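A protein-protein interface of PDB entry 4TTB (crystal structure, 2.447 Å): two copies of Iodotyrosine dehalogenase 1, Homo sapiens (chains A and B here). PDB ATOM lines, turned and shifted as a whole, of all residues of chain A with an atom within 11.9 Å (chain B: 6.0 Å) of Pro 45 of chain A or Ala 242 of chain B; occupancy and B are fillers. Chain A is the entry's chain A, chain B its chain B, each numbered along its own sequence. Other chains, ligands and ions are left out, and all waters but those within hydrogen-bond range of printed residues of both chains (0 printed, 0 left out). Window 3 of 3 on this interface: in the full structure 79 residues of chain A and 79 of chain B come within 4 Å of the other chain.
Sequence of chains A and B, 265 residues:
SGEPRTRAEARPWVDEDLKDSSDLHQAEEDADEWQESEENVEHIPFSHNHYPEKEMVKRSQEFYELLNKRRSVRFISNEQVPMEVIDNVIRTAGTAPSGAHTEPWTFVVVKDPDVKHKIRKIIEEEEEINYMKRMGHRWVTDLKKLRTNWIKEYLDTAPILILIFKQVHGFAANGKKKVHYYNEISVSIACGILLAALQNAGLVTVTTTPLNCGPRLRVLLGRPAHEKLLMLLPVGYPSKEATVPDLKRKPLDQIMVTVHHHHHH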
ATOM      1  N   VAL A  41      13.260   0.885   2.283  1.00  0.00           N
ATOM      2  CA  VAL A  41      13.003  -0.552   2.351  1.00  0.00           C
ATOM      3  C   VAL A  41      13.215  -1.214   0.977  1.00  0.00           C
ATOM      4  O   VAL A  41      13.346  -0.522  -0.032  1.00  0.00           O
ATOM      5  CB  VAL A  41      11.589  -0.843   2.902  1.00  0.00           C
ATOM      6  CG1 VAL A  41      11.607  -2.093   3.775  1.00  0.00           C
ATOM      7  CG2 VAL A  41      11.082   0.350   3.705  1.00  0.00           C
ATOM      8  N   GLU A  42      13.223  -2.547   0.951  1.00  0.00           N
ATOM      9  CA  GLU A  42      13.725  -3.338  -0.185  1.00  0.00           C
ATOM     10  C   GLU A  42      12.943  -3.185  -1.502  1.00  0.00           C
ATOM     11  O   GLU A  42      11.772  -2.808  -1.496  1.00  0.00           O
ATOM     12  CB  GLU A  42      13.765  -4.815   0.212  1.00  0.00           C
ATOM     13  CG  GLU A  42      15.130  -5.470   0.079  1.00  0.00           C
ATOM     14  CD  GLU A  42      15.428  -5.891  -1.344  1.00  0.00           C
ATOM     15  OE1 GLU A  42      14.458  -6.103  -2.106  1.00  0.00           O
ATOM     16  OE2 GLU A  42      16.623  -6.002  -1.701  1.00  0.00           O
ATOM     17  N   HIS A  43      13.605  -3.476  -2.625  1.00  0.00           N
ATOM     18  CA  HIS A  43      12.991  -3.396  -3.956  1.00  0.00           C
ATOM     19  C   HIS A  43      13.345  -4.620  -4.798  1.00  0.00           C
ATOM     20  O   HIS A  43      14.502  -4.964  -4.922  1.00  0.00           O
ATOM     21  CB  HIS A  43      13.439  -2.128  -4.687  1.00  0.00           C
ATOM     22  CG  HIS A  43      12.942  -0.863  -4.059  1.00  0.00           C
ATOM     23  ND1 HIS A  43      11.844  -0.176  -4.535  1.00  0.00           N
ATOM     24  CD2 HIS A  43      13.389  -0.161  -2.989  1.00  0.00           C
ATOM     25  CE1 HIS A  43      11.635   0.893  -3.785  1.00  0.00           C
ATOM     26  NE2 HIS A  43      12.557   0.923  -2.840  1.00  0.00           N
ATOM     27  N   ILE A  44      12.345  -5.267  -5.393  1.00  0.00           N
ATOM     28  CA  ILE A  44      12.585  -6.510  -6.132  1.00  0.00           C
ATOM     29  C   ILE A  44      12.218  -6.413  -7.616  1.00  0.00           C
ATOM     30  O   ILE A  44      11.359  -5.629  -7.987  1.00  0.00           O
ATOM     31  CB  ILE A  44      11.822  -7.690  -5.502  1.00  0.00           C
ATOM     32  CG1 ILE A  44      10.319  -7.427  -5.542  1.00  0.00           C
ATOM     33  CG2 ILE A  44      12.302  -7.922  -4.073  1.00  0.00           C
ATOM     34  CD1 ILE A  44       9.483  -8.609  -5.140  1.00  0.00           C
ATOM     35  N   PRO A  45      12.895  -7.204  -8.464  1.00  0.00           N
ATOM     36  CA  PRO A  45      12.585  -7.277  -9.897  1.00  0.00           C
ATOM     37  C   PRO A  45      11.098  -7.527 -10.146  1.00  0.00           C
ATOM     38  O   PRO A  45      10.486  -8.265  -9.383  1.00  0.00           O
ATOM     39  CB  PRO A  45      13.402  -8.486 -10.374  1.00  0.00           C
ATOM     40  CG  PRO A  45      14.391  -8.844  -9.202  1.00  0.00           C
ATOM     41  CD  PRO A  45      14.221  -7.777  -8.157  1.00  0.00           C
ATOM     42  N   PHE A  46      10.530  -6.915 -11.185  1.00  0.00           N
ATOM     43  CA  PHE A  46       9.102  -7.096 -11.509  1.00  0.00           C
ATOM     44  C   PHE A  46       8.876  -8.116 -12.641  1.00  0.00           C
ATOM     45  O   PHE A  46       9.505  -8.029 -13.703  1.00  0.00           O
ATOM     46  CB  PHE A  46       8.437  -5.755 -11.844  1.00  0.00           C
ATOM     47  CG  PHE A  46       7.002  -5.883 -12.265  1.00  0.00           C
ATOM     48  CD1 PHE A  46       6.026  -6.289 -11.360  1.00  0.00           C
ATOM     49  CD2 PHE A  46       6.617  -5.589 -13.568  1.00  0.00           C
ATOM     50  CE1 PHE A  46       4.719  -6.414 -11.747  1.00  0.00           C
ATOM     51  CE2 PHE A  46       5.315  -5.716 -13.954  1.00  0.00           C
ATOM     52  CZ  PHE A  46       4.356  -6.126 -13.045  1.00  0.00           C
ATOM     53  N   SER A  47       7.973  -9.073 -12.411  1.00  0.00           N
ATOM     54  CA  SER A  47       7.699 -10.151 -13.366  1.00  0.00           C
ATOM     55  C   SER A  47       7.094  -9.646 -14.677  1.00  0.00           C
ATOM     56  O   SER A  47       6.046  -8.997 -14.673  1.00  0.00           O
ATOM     57  CB  SER A  47       6.732 -11.163 -12.741  1.00  0.00           C
ATOM     58  OG  SER A  47       5.432 -10.603 -12.582  1.00  0.00           O
ATOM     59  N   HIS A  48       7.743  -9.965 -15.794  1.00  0.00           N
ATOM     60  CA  HIS A  48       7.294  -9.532 -17.117  1.00  0.00           C
ATOM     61  C   HIS A  48       5.883  -9.991 -17.514  1.00  0.00           C
ATOM     62  O   HIS A  48       4.957  -9.177 -17.561  1.00  0.00           O
ATOM     63  CB  HIS A  48       8.305  -9.969 -18.182  1.00  0.00           C
ATOM     64  CG  HIS A  48       8.201  -9.201 -19.463  1.00  0.00           C
ATOM     65  ND1 HIS A  48       9.063  -9.398 -20.521  1.00  0.00           N
ATOM     66  CD2 HIS A  48       7.342  -8.231 -19.854  1.00  0.00           C
ATOM     67  CE1 HIS A  48       8.737  -8.584 -21.509  1.00  0.00           C
ATOM     68  NE2 HIS A  48       7.696  -7.866 -21.130  1.00  0.00           N
ATOM     69  N   ASN A  49       5.733 -11.291 -17.778  1.00  0.00           N
ATOM     70  CA  ASN A  49       4.470 -11.873 -18.256  1.00  0.00           C
ATOM     71  C   ASN A  49       3.943 -11.210 -19.545  1.00  0.00           C
ATOM     72  O   ASN A  49       2.894 -10.552 -19.525  1.00  0.00           O
ATOM     73  CB  ASN A  49       3.400 -11.829 -17.146  1.00  0.00           C
ATOM     74  CG  ASN A  49       2.300 -12.880 -17.329  1.00  0.00           C
ATOM     75  OD1 ASN A  49       2.002 -13.302 -18.449  1.00  0.00           O
ATOM     76  ND2 ASN A  49       1.693 -13.301 -16.220  1.00  0.00           N
ATOM     77  N   VAL B  73       3.893   0.236 -11.152  1.00  0.00           N
ATOM     78  CA  VAL B  73       5.225   0.110 -11.719  1.00  0.00           C
ATOM     79  C   VAL B  73       5.704   1.476 -12.153  1.00  0.00           C
ATOM     80  O   VAL B  73       5.085   2.120 -12.995  1.00  0.00           O
ATOM     81  CB  VAL B  73       5.202  -0.799 -12.928  1.00  0.00           C
ATOM     82  CG1 VAL B  73       6.552  -0.829 -13.592  1.00  0.00           C
ATOM     83  CG2 VAL B  73       4.751  -2.193 -12.518  1.00  0.00           C
ATOM     84  N   PHE B  75       8.545   2.272 -13.578  1.00  0.00           N
ATOM     85  CA  PHE B  75       9.530   2.205 -14.649  1.00  0.00           C
ATOM     86  C   PHE B  75       8.878   1.678 -15.924  1.00  0.00           C
ATOM     87  O   PHE B  75       8.574   0.497 -16.030  1.00  0.00           O
ATOM     88  CB  PHE B  75      10.643   1.258 -14.214  1.00  0.00           C
ATOM     89  CG  PHE B  75      11.333   1.681 -12.935  1.00  0.00           C
ATOM     90  CD1 PHE B  75      12.593   2.259 -12.971  1.00  0.00           C
ATOM     91  CD2 PHE B  75      10.715   1.508 -11.698  1.00  0.00           C
ATOM     92  CE1 PHE B  75      13.227   2.665 -11.800  1.00  0.00           C
ATOM     93  CE2 PHE B  75      11.344   1.914 -10.518  1.00  0.00           C
ATOM     94  CZ  PHE B  75      12.596   2.490 -10.572  1.00  0.00           C
ATOM     95  N   ILE B  76       8.739   2.537 -16.927  1.00  0.00           N
ATOM     96  CA  ILE B  76       7.874   2.232 -18.059  1.00  0.00           C
ATOM     97  C   ILE B  76       8.514   2.484 -19.421  1.00  0.00           C
ATOM     98  O   ILE B  76       8.997   3.579 -19.709  1.00  0.00           O
ATOM     99  CB  ILE B  76       6.526   3.005 -17.966  1.00  0.00           C
ATOM    100  CG1 ILE B  76       5.741   2.565 -16.728  1.00  0.00           C
ATOM    101  CG2 ILE B  76       5.670   2.774 -19.212  1.00  0.00           C
ATOM    102  CD1 ILE B  76       4.641   3.505 -16.346  1.00  0.00           C
ATOM    103  N   PRO B 238       6.287  -2.353 -18.823  1.00  0.00           N
ATOM    104  CA  PRO B 238       7.374  -2.166 -17.862  1.00  0.00           C
ATOM    105  C   PRO B 238       8.776  -2.235 -18.512  1.00  0.00           C
ATOM    106  O   PRO B 238       8.979  -2.979 -19.474  1.00  0.00           O
ATOM    107  CB  PRO B 238       7.177  -3.344 -16.900  1.00  0.00           C
ATOM    108  CG  PRO B 238       6.510  -4.395 -17.720  1.00  0.00           C
ATOM    109  CD  PRO B 238       5.555  -3.609 -18.589  1.00  0.00           C
ATOM    110  N   SER B 239       9.720  -1.453 -17.983  1.00  0.00           N
ATOM    111  CA  SER B 239      11.129  -1.521 -18.372  1.00  0.00           C
ATOM    112  C   SER B 239      11.777  -2.823 -17.929  1.00  0.00           C
ATOM    113  O   SER B 239      11.308  -3.481 -17.007  1.00  0.00           O
ATOM    114  CB  SER B 239      11.909  -0.370 -17.735  1.00  0.00           C
ATOM    115  OG  SER B 239      11.849   0.795 -18.531  1.00  0.00           O
ATOM    116  N   LYS B 240      12.877  -3.174 -18.585  1.00  0.00           N
ATOM    117  CA  LYS B 240      13.690  -4.324 -18.201  1.00  0.00           C
ATOM    118  C   LYS B 240      14.209  -4.181 -16.765  1.00  0.00           C
ATOM    119  O   LYS B 240      14.282  -5.154 -16.008  1.00  0.00           O
ATOM    120  CB  LYS B 240      14.862  -4.466 -19.164  1.00  0.00           C
ATOM    121  CG  LYS B 240      15.315  -5.892 -19.366  1.00  0.00           C
ATOM    122  CD  LYS B 240      14.157  -6.746 -19.840  1.00  0.00           C
ATOM    123  CE  LYS B 240      14.560  -8.206 -19.925  1.00  0.00           C
ATOM    124  NZ  LYS B 240      13.385  -9.058 -20.256  1.00  0.00           N
ATOM    125  N   GLU B 241      14.533  -2.951 -16.391  1.00  0.00           N
ATOM    126  CA  GLU B 241      15.093  -2.661 -15.081  1.00  0.00           C
ATOM    127  C   GLU B 241      14.016  -2.398 -14.039  1.00  0.00           C
ATOM    128  O   GLU B 241      14.323  -2.068 -12.899  1.00  0.00           O
ATOM    129  CB  GLU B 241      15.928  -1.405 -15.187  1.00  0.00           C
ATOM    130  CG  GLU B 241      15.087  -0.242 -15.648  1.00  0.00           C
ATOM    131  CD  GLU B 241      15.868   1.037 -15.722  1.00  0.00           C
ATOM    132  OE1 GLU B 241      17.122   0.985 -15.602  1.00  0.00           O
ATOM    133  OE2 GLU B 241      15.222   2.094 -15.898  1.00  0.00           O
ATOM    134  N   ALA B 242      12.760  -2.520 -14.432  1.00  0.00           N
ATOM    135  CA  ALA B 242      11.673  -2.178 -13.538  1.00  0.00           C
ATOM    136  C   ALA B 242      11.683  -3.047 -12.297  1.00  0.00           C
ATOM    137  O   ALA B 242      11.741  -4.272 -12.373  1.00  0.00           O
ATOM    138  CB  ALA B 242      10.309  -2.260 -14.256  1.00  0.00           C
ATOM    139  N   THR B 243      11.650  -2.389 -11.150  1.00  0.00           N
ATOM    140  CA  THR B 243      11.476  -3.077  -9.892  1.00  0.00           C
ATOM    141  C   THR B 243      10.191  -2.595  -9.265  1.00  0.00           C
ATOM    142  O   THR B 243       9.512  -1.696  -9.787  1.00  0.00           O
ATOM    143  CB  THR B 243      12.612  -2.750  -8.902  1.00  0.00           C
ATOM    144  OG1 THR B 243      12.670  -1.333  -8.703  1.00  0.00           O
ATOM    145  CG2 THR B 243      13.933  -3.230  -9.428  1.00  0.00           C
ATOM    146  N   VAL B 244       9.865  -3.188  -8.126  1.00  0.00           N
ATOM    147  CA  VAL B 244       8.732  -2.744  -7.339  1.00  0.00           C
ATOM    148  C   VAL B 244       9.183  -2.920  -5.916  1.00  0.00           C
ATOM    149  O   VAL B 244       9.932  -3.851  -5.619  1.00  0.00           O
ATOM    150  CB  VAL B 244       7.425  -3.573  -7.625  1.00  0.00           C
ATOM    151  CG1 VAL B 244       6.956  -3.379  -9.046  1.00  0.00           C
ATOM    152  CG2 VAL B 244       7.633  -5.052  -7.359  1.00  0.00           C
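The backbone NH of Ile 44 of chain A sits at hydrogen-bond distance from the backbone carbonyl oxygen of Val 244 of chain B, 2.8 Å away.
O of Ala 242 of chain B is in hydrogen-bond range of N of Phe 46 of chain A, at 3.1 Å.
The backbone carbonyl oxygen of Val 41 of chain A lies close to a ring nitrogen (NE2) of His 43 of chain A (3.3 Å).
Among the printed residues, pairs that only touch across the chains: His 43 of chain A with Val 244 of chain B, Ile 44 of chain A with Thr 243 of chain B, Pro 45 of chain A with Ala 242 of chain B, Phe 46 of chain A with Val 73 of chain B and Phe 46 of chain A with Val 244 of chain B.
Glu 42 of chain A touches none of the printed residues of chain B.
Of the printed residues of chain B, His 43 of chain A touches Val 244 (3.5 Å).
Of the printed residues of chain B, Ile 44 of chain A touches Thr 243 and Val 244.
Of the printed residues of chain B, Pro 45 of chain A touches Ala 242 (3.98 Å).
Of the printed residues of chain B, Phe 46 of chain A touches Val 73 (3.8 Å), Ala 242 (3.1 Å) and Val 244 (3.8 Å).
Of chain A, only Phe 46 comes within 4 Å of Val 73 of chain B.
No residue of chain A comes within 4 Å of Phe 75 of chain B.
No residue of chain A comes within 4 Å of Pro 238 of chain B.
No residue of chain A comes within 4 Å of Glu 241 of chain B.
Of the printed residues of chain A, Ala 242 of chain B touches Pro 45 and Phe 46.
Thr 243 of chain B touches just one residue of chain A: Ile 44 (3.2 Å).
Printed residues of chain A within 4 Å of Val 244 of chain B: His 43, Ile 44 and Phe 46.
The nearest printed residue of chain B that does not touch Pro 45 of chain A is Thr 243 of chain B (4.2 Å).
The nearest printed residue of chain A that does not touch Ala 242 of chain B is Ile 44 of chain A (4.6 Å).
The nearest printed residue of chain B that does not touch Ile 44 of chain A is Ala 242 of chain B (4.6 Å).
Hydrophobic or aromatic side chains of chain A that line the printed part of chain B: Ile 44 and Phe 46.
Hydrophobic or aromatic side chains of chain B within 4 Å of the printed part of chain A: Val 73 and Val 244.
Along chain B the printed residues that touch a printed residue of chain A span positions 73 to 244.
Among the printed residues, no Asp or Glu carboxylate lies within 4 Å of a Lys or Arg side-chain nitrogen of the other chain.
No position is printed for both chains.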
